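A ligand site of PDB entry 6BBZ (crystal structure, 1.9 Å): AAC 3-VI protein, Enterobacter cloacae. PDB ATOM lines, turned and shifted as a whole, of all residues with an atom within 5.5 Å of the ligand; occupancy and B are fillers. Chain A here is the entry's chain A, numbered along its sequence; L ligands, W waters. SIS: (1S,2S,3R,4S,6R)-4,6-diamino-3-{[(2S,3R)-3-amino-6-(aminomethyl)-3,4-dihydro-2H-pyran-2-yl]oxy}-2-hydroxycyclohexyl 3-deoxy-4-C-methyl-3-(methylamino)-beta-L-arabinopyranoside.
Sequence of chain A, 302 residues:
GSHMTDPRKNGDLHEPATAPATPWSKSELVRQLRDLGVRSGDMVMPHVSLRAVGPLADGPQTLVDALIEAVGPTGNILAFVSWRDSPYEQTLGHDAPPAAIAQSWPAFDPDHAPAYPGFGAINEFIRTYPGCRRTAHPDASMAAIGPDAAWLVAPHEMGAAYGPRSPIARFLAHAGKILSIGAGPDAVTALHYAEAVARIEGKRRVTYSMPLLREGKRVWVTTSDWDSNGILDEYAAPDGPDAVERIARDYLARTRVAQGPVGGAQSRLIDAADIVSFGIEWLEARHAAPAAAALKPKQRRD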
ATOM      1  N   PHE A  80      10.259  -7.090 -21.465  1.00  0.00           N
ATOM      2  CA  PHE A  80      10.999  -7.934 -22.411  1.00  0.00           C
ATOM      3  C   PHE A  80      10.767  -7.332 -23.798  1.00  0.00           C
ATOM      4  O   PHE A  80       9.681  -7.475 -24.372  1.00  0.00           O
ATOM      5  CB  PHE A  80      10.540  -9.387 -22.304  1.00  0.00           C
ATOM      6  CG  PHE A  80      11.101 -10.299 -23.376  1.00  0.00           C
ATOM      7  CD1 PHE A  80      10.281 -11.229 -24.008  1.00  0.00           C
ATOM      8  CD2 PHE A  80      12.429 -10.231 -23.758  1.00  0.00           C
ATOM      9  CE1 PHE A  80      10.798 -12.076 -24.990  1.00  0.00           C
ATOM     10  CE2 PHE A  80      12.940 -11.057 -24.760  1.00  0.00           C
ATOM     11  CZ  PHE A  80      12.134 -11.980 -25.364  1.00  0.00           C
ATOM     12  N   SER A  82      13.355  -7.229 -26.570  1.00  0.00           N
ATOM     13  CA  SER A  82      14.077  -7.927 -27.639  1.00  0.00           C
ATOM     14  C   SER A  82      14.544  -6.903 -28.672  1.00  0.00           C
ATOM     15  O   SER A  82      14.834  -5.734 -28.349  1.00  0.00           O
ATOM     16  CB  SER A  82      13.224  -9.021 -28.196  1.00  0.00           C
ATOM     17  OG  SER A  82      13.929  -9.818 -29.125  1.00  0.00           O
ATOM     18  N   TRP A  83      14.610  -7.310 -29.931  1.00  0.00           N
ATOM     19  CA  TRP A  83      15.207  -6.496 -30.974  1.00  0.00           C
ATOM     20  C   TRP A  83      14.538  -6.819 -32.298  1.00  0.00           C
ATOM     21  O   TRP A  83      14.561  -7.978 -32.712  1.00  0.00           O
ATOM     22  CB  TRP A  83      16.696  -6.755 -31.043  1.00  0.00           C
ATOM     23  CG  TRP A  83      17.429  -6.056 -32.149  1.00  0.00           C
ATOM     24  CD1 TRP A  83      17.043  -4.930 -32.812  1.00  0.00           C
ATOM     25  CD2 TRP A  83      18.675  -6.458 -32.710  1.00  0.00           C
ATOM     26  NE1 TRP A  83      17.993  -4.598 -33.756  1.00  0.00           N
ATOM     27  CE2 TRP A  83      19.003  -5.526 -33.708  1.00  0.00           C
ATOM     28  CE3 TRP A  83      19.555  -7.513 -32.453  1.00  0.00           C
ATOM     29  CZ2 TRP A  83      20.165  -5.616 -34.463  1.00  0.00           C
ATOM     30  CZ3 TRP A  83      20.707  -7.602 -33.199  1.00  0.00           C
ATOM     31  CH2 TRP A  83      21.012  -6.661 -34.191  1.00  0.00           C
ATOM     32  N   SER A  86      16.807  -8.946 -34.606  1.00  0.00           N
ATOM     33  CA  SER A  86      17.628 -10.019 -34.094  1.00  0.00           C
ATOM     34  C   SER A  86      17.838 -11.071 -35.191  1.00  0.00           C
ATOM     35  O   SER A  86      16.854 -11.577 -35.741  1.00  0.00           O
ATOM     36  CB  SER A  86      16.970 -10.670 -32.894  1.00  0.00           C
ATOM     37  OG  SER A  86      17.763 -11.751 -32.449  1.00  0.00           O
ATOM     38  N   TYR A  88      18.196 -14.158 -35.168  1.00  0.00           N
ATOM     39  CA  TYR A  88      18.079 -15.445 -34.496  1.00  0.00           C
ATOM     40  C   TYR A  88      17.852 -16.574 -35.494  1.00  0.00           C
ATOM     41  O   TYR A  88      18.619 -17.533 -35.543  1.00  0.00           O
ATOM     42  CB  TYR A  88      16.936 -15.357 -33.471  1.00  0.00           C
ATOM     43  CG  TYR A  88      16.714 -16.591 -32.634  1.00  0.00           C
ATOM     44  CD1 TYR A  88      17.323 -16.729 -31.389  1.00  0.00           C
ATOM     45  CD2 TYR A  88      15.888 -17.611 -33.081  1.00  0.00           C
ATOM     46  CE1 TYR A  88      17.107 -17.852 -30.605  1.00  0.00           C
ATOM     47  CE2 TYR A  88      15.660 -18.740 -32.300  1.00  0.00           C
ATOM     48  CZ  TYR A  88      16.274 -18.865 -31.073  1.00  0.00           C
ATOM     49  OH  TYR A  88      16.065 -19.982 -30.294  1.00  0.00           O
ATOM     50  N   GLU A  89      16.814 -16.442 -36.332  1.00  0.00           N
ATOM     51  CA  GLU A  89      16.516 -17.485 -37.307  1.00  0.00           C
ATOM     52  C   GLU A  89      17.697 -17.721 -38.251  1.00  0.00           C
ATOM     53  O   GLU A  89      17.994 -18.859 -38.605  1.00  0.00           O
ATOM     54  CB  GLU A  89      15.268 -17.126 -38.110  1.00  0.00           C
ATOM     55  CG  GLU A  89      13.982 -17.137 -37.332  1.00  0.00           C
ATOM     56  CD  GLU A  89      13.614 -15.774 -36.732  1.00  0.00           C
ATOM     57  OE1 GLU A  89      14.477 -14.861 -36.668  1.00  0.00           O
ATOM     58  OE2 GLU A  89      12.453 -15.643 -36.314  1.00  0.00           O
ATOM     59  N   TYR A 116      11.230  -5.679 -30.598  1.00  0.00           N
ATOM     60  CA  TYR A 116      10.640  -6.684 -31.474  1.00  0.00           C
ATOM     61  C   TYR A 116       9.126  -6.553 -31.439  1.00  0.00           C
ATOM     62  O   TYR A 116       8.522  -6.711 -30.373  1.00  0.00           O
ATOM     63  CB  TYR A 116      11.056  -8.095 -31.065  1.00  0.00           C
ATOM     64  CG  TYR A 116      10.538  -9.146 -32.014  1.00  0.00           C
ATOM     65  CD1 TYR A 116      11.125  -9.343 -33.257  1.00  0.00           C
ATOM     66  CD2 TYR A 116       9.442  -9.934 -31.688  1.00  0.00           C
ATOM     67  CE1 TYR A 116      10.650 -10.301 -34.136  1.00  0.00           C
ATOM     68  CE2 TYR A 116       8.956 -10.891 -32.558  1.00  0.00           C
ATOM     69  CZ  TYR A 116       9.565 -11.061 -33.779  1.00  0.00           C
ATOM     70  OH  TYR A 116       9.085 -12.012 -34.653  1.00  0.00           O
ATOM     71  N   PHE A 119       6.255  -9.023 -29.639  1.00  0.00           N
ATOM     72  CA  PHE A 119       6.101  -9.147 -28.192  1.00  0.00           C
ATOM     73  C   PHE A 119       5.267  -8.027 -27.603  1.00  0.00           C
ATOM     74  O   PHE A 119       5.134  -7.942 -26.374  1.00  0.00           O
ATOM     75  CB  PHE A 119       7.470  -9.223 -27.509  1.00  0.00           C
ATOM     76  CG  PHE A 119       8.315 -10.394 -27.966  1.00  0.00           C
ATOM     77  CD1 PHE A 119       7.712 -11.593 -28.305  1.00  0.00           C
ATOM     78  CD2 PHE A 119       9.683 -10.289 -28.082  1.00  0.00           C
ATOM     79  CE1 PHE A 119       8.474 -12.670 -28.743  1.00  0.00           C
ATOM     80  CE2 PHE A 119      10.435 -11.351 -28.511  1.00  0.00           C
ATOM     81  CZ  PHE A 119       9.834 -12.542 -28.838  1.00  0.00           C
ATOM     82  N   ASP A 139      19.038 -10.513 -28.357  1.00  0.00           N
ATOM     83  CA  ASP A 139      17.800 -11.224 -28.625  1.00  0.00           C
ATOM     84  C   ASP A 139      16.865 -11.232 -27.424  1.00  0.00           C
ATOM     85  O   ASP A 139      15.632 -11.235 -27.586  1.00  0.00           O
ATOM     86  CB  ASP A 139      18.099 -12.651 -29.066  1.00  0.00           C
ATOM     87  CG  ASP A 139      16.862 -13.352 -29.567  1.00  0.00           C
ATOM     88  OD1 ASP A 139      16.290 -12.930 -30.601  1.00  0.00           O
ATOM     89  OD2 ASP A 139      16.435 -14.297 -28.877  1.00  0.00           O
ATOM     90  N   TYR A 162      17.486 -15.986 -19.956  1.00  0.00           N
ATOM     91  CA  TYR A 162      16.379 -15.898 -19.013  1.00  0.00           C
ATOM     92  C   TYR A 162      16.656 -16.593 -17.691  1.00  0.00           C
ATOM     93  O   TYR A 162      15.773 -16.643 -16.833  1.00  0.00           O
ATOM     94  CB  TYR A 162      15.102 -16.495 -19.635  1.00  0.00           C
ATOM     95  CG  TYR A 162      14.836 -15.940 -21.022  1.00  0.00           C
ATOM     96  CD1 TYR A 162      15.087 -16.699 -22.158  1.00  0.00           C
ATOM     97  CD2 TYR A 162      14.374 -14.648 -21.190  1.00  0.00           C
ATOM     98  CE1 TYR A 162      14.867 -16.178 -23.428  1.00  0.00           C
ATOM     99  CE2 TYR A 162      14.145 -14.119 -22.439  1.00  0.00           C
ATOM    100  CZ  TYR A 162      14.403 -14.884 -23.555  1.00  0.00           C
ATOM    101  OH  TYR A 162      14.182 -14.341 -24.798  1.00  0.00           O
ATOM    102  N   ASP A 186       0.585 -17.790 -22.661  1.00  0.00           N
ATOM    103  CA  ASP A 186       1.867 -18.064 -23.299  1.00  0.00           C
ATOM    104  C   ASP A 186       2.874 -16.925 -23.154  1.00  0.00           C
ATOM    105  O   ASP A 186       4.054 -17.110 -23.472  1.00  0.00           O
ATOM    106  CB  ASP A 186       1.655 -18.336 -24.792  1.00  0.00           C
ATOM    107  CG  ASP A 186       1.067 -17.145 -25.520  1.00  0.00           C
ATOM    108  OD1 ASP A 186      -0.010 -16.673 -25.111  1.00  0.00           O
ATOM    109  OD2 ASP A 186       1.682 -16.686 -26.509  1.00  0.00           O
ATOM    110  N   ALA A 187       2.448 -15.756 -22.692  1.00  0.00           N
ATOM    111  CA  ALA A 187       3.287 -14.569 -22.757  1.00  0.00           C
ATOM    112  C   ALA A 187       4.172 -14.363 -21.523  1.00  0.00           C
ATOM    113  O   ALA A 187       4.909 -13.368 -21.469  1.00  0.00           O
ATOM    114  CB  ALA A 187       2.403 -13.335 -22.992  1.00  0.00           C
ATOM    115  N   HIS A 192      10.480 -18.777 -18.394  1.00  0.00           N
ATOM    116  CA  HIS A 192      11.678 -19.368 -18.972  1.00  0.00           C
ATOM    117  C   HIS A 192      12.791 -19.540 -17.950  1.00  0.00           C
ATOM    118  O   HIS A 192      13.686 -20.356 -18.167  1.00  0.00           O
ATOM    119  CB  HIS A 192      12.148 -18.544 -20.182  1.00  0.00           C
ATOM    120  CG  HIS A 192      11.229 -18.680 -21.346  1.00  0.00           C
ATOM    121  ND1 HIS A 192      10.967 -19.899 -21.928  1.00  0.00           N
ATOM    122  CD2 HIS A 192      10.498 -17.764 -22.015  1.00  0.00           C
ATOM    123  CE1 HIS A 192      10.113 -19.727 -22.917  1.00  0.00           C
ATOM    124  NE2 HIS A 192       9.814 -18.446 -22.999  1.00  0.00           N
ATOM    125  N   SER A 228      14.319 -21.428 -25.906  1.00  0.00           N
ATOM    126  CA  SER A 228      13.156 -20.716 -25.394  1.00  0.00           C
ATOM    127  C   SER A 228      11.903 -20.949 -26.233  1.00  0.00           C
ATOM    128  O   SER A 228      10.859 -20.364 -25.925  1.00  0.00           O
ATOM    129  CB  SER A 228      13.436 -19.210 -25.325  1.00  0.00           C
ATOM    130  OG  SER A 228      13.573 -18.651 -26.616  1.00  0.00           O
ATOM    131  N   ASN A 229      11.976 -21.759 -27.288  1.00  0.00           N
ATOM    132  CA  ASN A 229      10.808 -22.104 -28.084  1.00  0.00           C
ATOM    133  C   ASN A 229      10.340 -23.534 -27.813  1.00  0.00           C
ATOM    134  O   ASN A 229       9.599 -24.109 -28.605  1.00  0.00           O
ATOM    135  CB  ASN A 229      11.118 -21.904 -29.567  1.00  0.00           C
ATOM    136  CG  ASN A 229      10.973 -20.447 -29.992  1.00  0.00           C
ATOM    137  OD1 ASN A 229       9.927 -19.853 -29.799  1.00  0.00           O
ATOM    138  ND2 ASN A 229      12.031 -19.879 -30.553  1.00  0.00           N
ATOM    139  N   GLY A 230      10.771 -24.103 -26.693  1.00  0.00           N
ATOM    140  CA  GLY A 230      10.334 -25.430 -26.289  1.00  0.00           C
ATOM    141  C   GLY A 230      11.449 -26.143 -25.557  1.00  0.00           C
ATOM    142  O   GLY A 230      12.422 -26.565 -26.177  1.00  0.00           O
ATOM    143  N   TYR A 235       7.148 -29.921 -26.022  1.00  0.00           N
ATOM    144  CA  TYR A 235       6.700 -28.538 -25.888  1.00  0.00           C
ATOM    145  C   TYR A 235       7.179 -27.662 -27.038  1.00  0.00           C
ATOM    146  O   TYR A 235       6.969 -26.448 -27.014  1.00  0.00           O
ATOM    147  CB  TYR A 235       7.172 -27.969 -24.550  1.00  0.00           C
ATOM    148  CG  TYR A 235       6.763 -28.770 -23.338  1.00  0.00           C
ATOM    149  CD1 TYR A 235       7.721 -29.292 -22.470  1.00  0.00           C
ATOM    150  CD2 TYR A 235       5.429 -29.021 -23.060  1.00  0.00           C
ATOM    151  CE1 TYR A 235       7.363 -30.017 -21.363  1.00  0.00           C
ATOM    152  CE2 TYR A 235       5.053 -29.765 -21.939  1.00  0.00           C
ATOM    153  CZ  TYR A 235       6.023 -30.253 -21.093  1.00  0.00           C
ATOM    154  OH  TYR A 235       5.675 -30.994 -19.995  1.00  0.00           O
ATOM    155  N   ALA A 237       6.518 -28.028 -30.460  1.00  0.00           N
ATOM    156  CA  ALA A 237       5.729 -27.915 -31.673  1.00  0.00           C
ATOM    157  C   ALA A 237       5.566 -26.447 -32.043  1.00  0.00           C
ATOM    158  O   ALA A 237       5.403 -25.601 -31.159  1.00  0.00           O
ATOM    159  CB  ALA A 237       4.355 -28.578 -31.490  1.00  0.00           C
ATOM    160  N   PRO A 238       5.600 -26.100 -33.347  1.00  0.00           N
ATOM    161  CA  PRO A 238       5.653 -24.672 -33.729  1.00  0.00           C
ATOM    162  C   PRO A 238       4.424 -23.913 -33.237  1.00  0.00           C
ATOM    163  O   PRO A 238       4.542 -22.895 -32.542  1.00  0.00           O
ATOM    164  CB  PRO A 238       5.746 -24.717 -35.246  1.00  0.00           C
ATOM    165  CG  PRO A 238       5.113 -26.008 -35.641  1.00  0.00           C
ATOM    166  CD  PRO A 238       5.374 -26.973 -34.507  1.00  0.00           C
ATOM    167  N   GLY A 240       2.097 -24.015 -30.383  1.00  0.00           N
ATOM    168  CA  GLY A 240       2.224 -24.531 -29.036  1.00  0.00           C
ATOM    169  C   GLY A 240       1.327 -25.732 -28.795  1.00  0.00           C
ATOM    170  O   GLY A 240       0.953 -26.453 -29.712  1.00  0.00           O
ATOM    171  N   ASP A 242       3.533 -24.491 -25.562  1.00  0.00           N
ATOM    172  CA  ASP A 242       4.830 -24.728 -24.953  1.00  0.00           C
ATOM    173  C   ASP A 242       4.635 -24.959 -23.449  1.00  0.00           C
ATOM    174  O   ASP A 242       3.515 -24.975 -22.927  1.00  0.00           O
ATOM    175  CB  ASP A 242       5.779 -23.578 -25.279  1.00  0.00           C
ATOM    176  CG  ASP A 242       5.400 -22.241 -24.644  1.00  0.00           C
ATOM    177  OD1 ASP A 242       6.262 -21.339 -24.657  1.00  0.00           O
ATOM    178  OD2 ASP A 242       4.271 -22.081 -24.148  1.00  0.00           O
ATOM    179  N   VAL A 244       5.632 -22.980 -21.054  1.00  0.00           N
ATOM    180  CA  VAL A 244       5.173 -21.756 -20.396  1.00  0.00           C
ATOM    181  C   VAL A 244       3.656 -21.744 -20.335  1.00  0.00           C
ATOM    182  O   VAL A 244       3.054 -21.568 -19.262  1.00  0.00           O
ATOM    183  CB  VAL A 244       5.723 -20.518 -21.128  1.00  0.00           C
ATOM    184  CG1 VAL A 244       5.164 -19.216 -20.514  1.00  0.00           C
ATOM    185  CG2 VAL A 244       7.244 -20.512 -21.100  1.00  0.00           C
HETATM  186  C11 SIS L   1       6.403 -17.634 -28.528  1.00  0.00           C
HETATM  187  C12 SIS L   1      11.153 -16.036 -27.025  1.00  0.00           C
HETATM  188  C13 SIS L   1      12.581 -16.306 -30.003  1.00  0.00           C
HETATM  189  C21 SIS L   1       5.146 -17.063 -28.485  1.00  0.00           C
HETATM  190  C22 SIS L   1      10.418 -16.809 -25.854  1.00  0.00           C
HETATM  191  C23 SIS L   1      13.499 -15.142 -30.392  1.00  0.00           C
HETATM  192  C31 SIS L   1       4.322 -17.935 -29.541  1.00  0.00           C
HETATM  193  C32 SIS L   1       8.862 -16.706 -26.032  1.00  0.00           C
HETATM  194  C33 SIS L   1      12.806 -14.238 -31.379  1.00  0.00           C
HETATM  195  C41 SIS L   1       4.792 -19.244 -29.861  1.00  0.00           C
HETATM  196  C42 SIS L   1       8.472 -17.291 -27.412  1.00  0.00           C
HETATM  197  C43 SIS L   1      12.315 -14.997 -32.576  1.00  0.00           C
HETATM  198  C51 SIS L   1       5.738 -19.993 -28.872  1.00  0.00           C
HETATM  199  C52 SIS L   1       9.377 -16.703 -28.572  1.00  0.00           C
HETATM  200  C53 SIS L   1      11.463 -16.216 -32.177  1.00  0.00           C
HETATM  201  C61 SIS L   1       5.949 -21.438 -28.826  1.00  0.00           C
HETATM  202  C62 SIS L   1      10.905 -16.645 -28.342  1.00  0.00           C
HETATM  203  C83 SIS L   1      11.424 -14.070 -33.449  1.00  0.00           C
HETATM  204  C93 SIS L   1      13.317 -11.789 -31.669  1.00  0.00           C
HETATM  205  N12 SIS L   1      12.587 -16.004 -26.782  1.00  0.00           N
HETATM  206  N21 SIS L   1       4.583 -17.170 -27.154  1.00  0.00           N
HETATM  207  N32 SIS L   1       8.141 -17.456 -25.081  1.00  0.00           N
HETATM  208  N33 SIS L   1      13.822 -13.171 -31.813  1.00  0.00           N
HETATM  209  N61 SIS L   1       7.422 -21.562 -28.800  1.00  0.00           N
HETATM  210  O11 SIS L   1       7.165 -16.826 -27.591  1.00  0.00           O
HETATM  211  O23 SIS L   1      13.860 -14.414 -29.192  1.00  0.00           O
HETATM  212  O43 SIS L   1      13.430 -15.461 -33.341  1.00  0.00           O
HETATM  213  O51 SIS L   1       6.446 -19.134 -28.019  1.00  0.00           O
HETATM  214  O52 SIS L   1       8.989 -16.981 -29.920  1.00  0.00           O
HETATM  215  O53 SIS L   1      12.174 -17.087 -31.206  1.00  0.00           O
HETATM  216  O62 SIS L   1      11.471 -15.793 -29.396  1.00  0.00           O
HETATM  217  O   HOH W   1       7.787 -14.374 -23.719  1.00  0.00           O
HETATM  218  O   HOH W   2      14.429 -12.659 -34.545  1.00  0.00           O
HETATM  219  O   HOH W   3       6.212 -24.398 -28.837  1.00  0.00           O
HETATM  220  O   HOH W   4       5.571 -18.839 -24.668  1.00  0.00           O
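The side-chain carboxylate (OD1) of Asp 139 is in salt-bridge range of a nitrogen (N33) of the ligand (2.8 Å).
A nitrogen (N12) of the ligand is in hydrogen-bond range of the side-chain hydroxyl (OG) of Ser 228 (2.8 Å).
NE2 of His 192 is in hydrogen-bond range of N32 of the ligand (2.8 Å).
A nitrogen (N61) of the ligand lies within hydrogen-bond range of the backbone carbonyl oxygen (O) of Asn 229, at 3.4 Å.
ND2 of Asn 229 sits at hydrogen-bond distance from O53 of the ligand, at 2.9 Å.
OD2 of Asp 186 lies within salt-bridge range of N21 of the ligand (3.0 Å).
OH of Tyr 162 is in hydrogen-bond range of N12 of the ligand (3.0 Å).
O43 of the ligand sits at hydrogen-bond distance from OE2 of Glu 89, at 3.1 Å.
The side-chain hydroxyl (OG) of Ser 82 sits at hydrogen-bond distance from the backbone carbonyl oxygen (O) of Asp 139, at 2.7 Å.
The side-chain carboxylate (OD1) of Asp 139 lies within hydrogen-bond range of the side-chain hydroxyl (OG) of Ser 86.
Ser 82 touches the ligand (OG to C93, 3.3 Å).
CD2 of Tyr 88 touches O43 of the ligand, 3.3 Å away.
Tyr 116 touches the ligand (OH to C83, 3.3 Å).
CZ of Phe 119 touches O62 of the ligand, at 3.7 Å.
Hydrophobic or aromatic side chains within 4 Å of the ligand: Tyr 88, Tyr 116, Phe 119, Tyr 162 and His 192.
11 residues have an atom within 4 Å of the ligand: Ser 82, Tyr 88, Glu 89, Tyr 116, Phe 119, Asp 139, Tyr 162, Asp 186, His 192, Ser 228 and Asn 229.
Water W2 lies within hydrogen-bond range of a nitrogen (N33) of the ligand, the backbone carbonyl oxygen of Ser 86 and the side-chain carboxylate of Glu 89.
Water W4 lies within hydrogen-bond range of the backbone carbonyl oxygen of Asp 186 (2.6 Å), the side-chain carboxylate of Asp 242 (2.6 Å) and a nitrogen (N32) of the ligand (2.9 Å).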
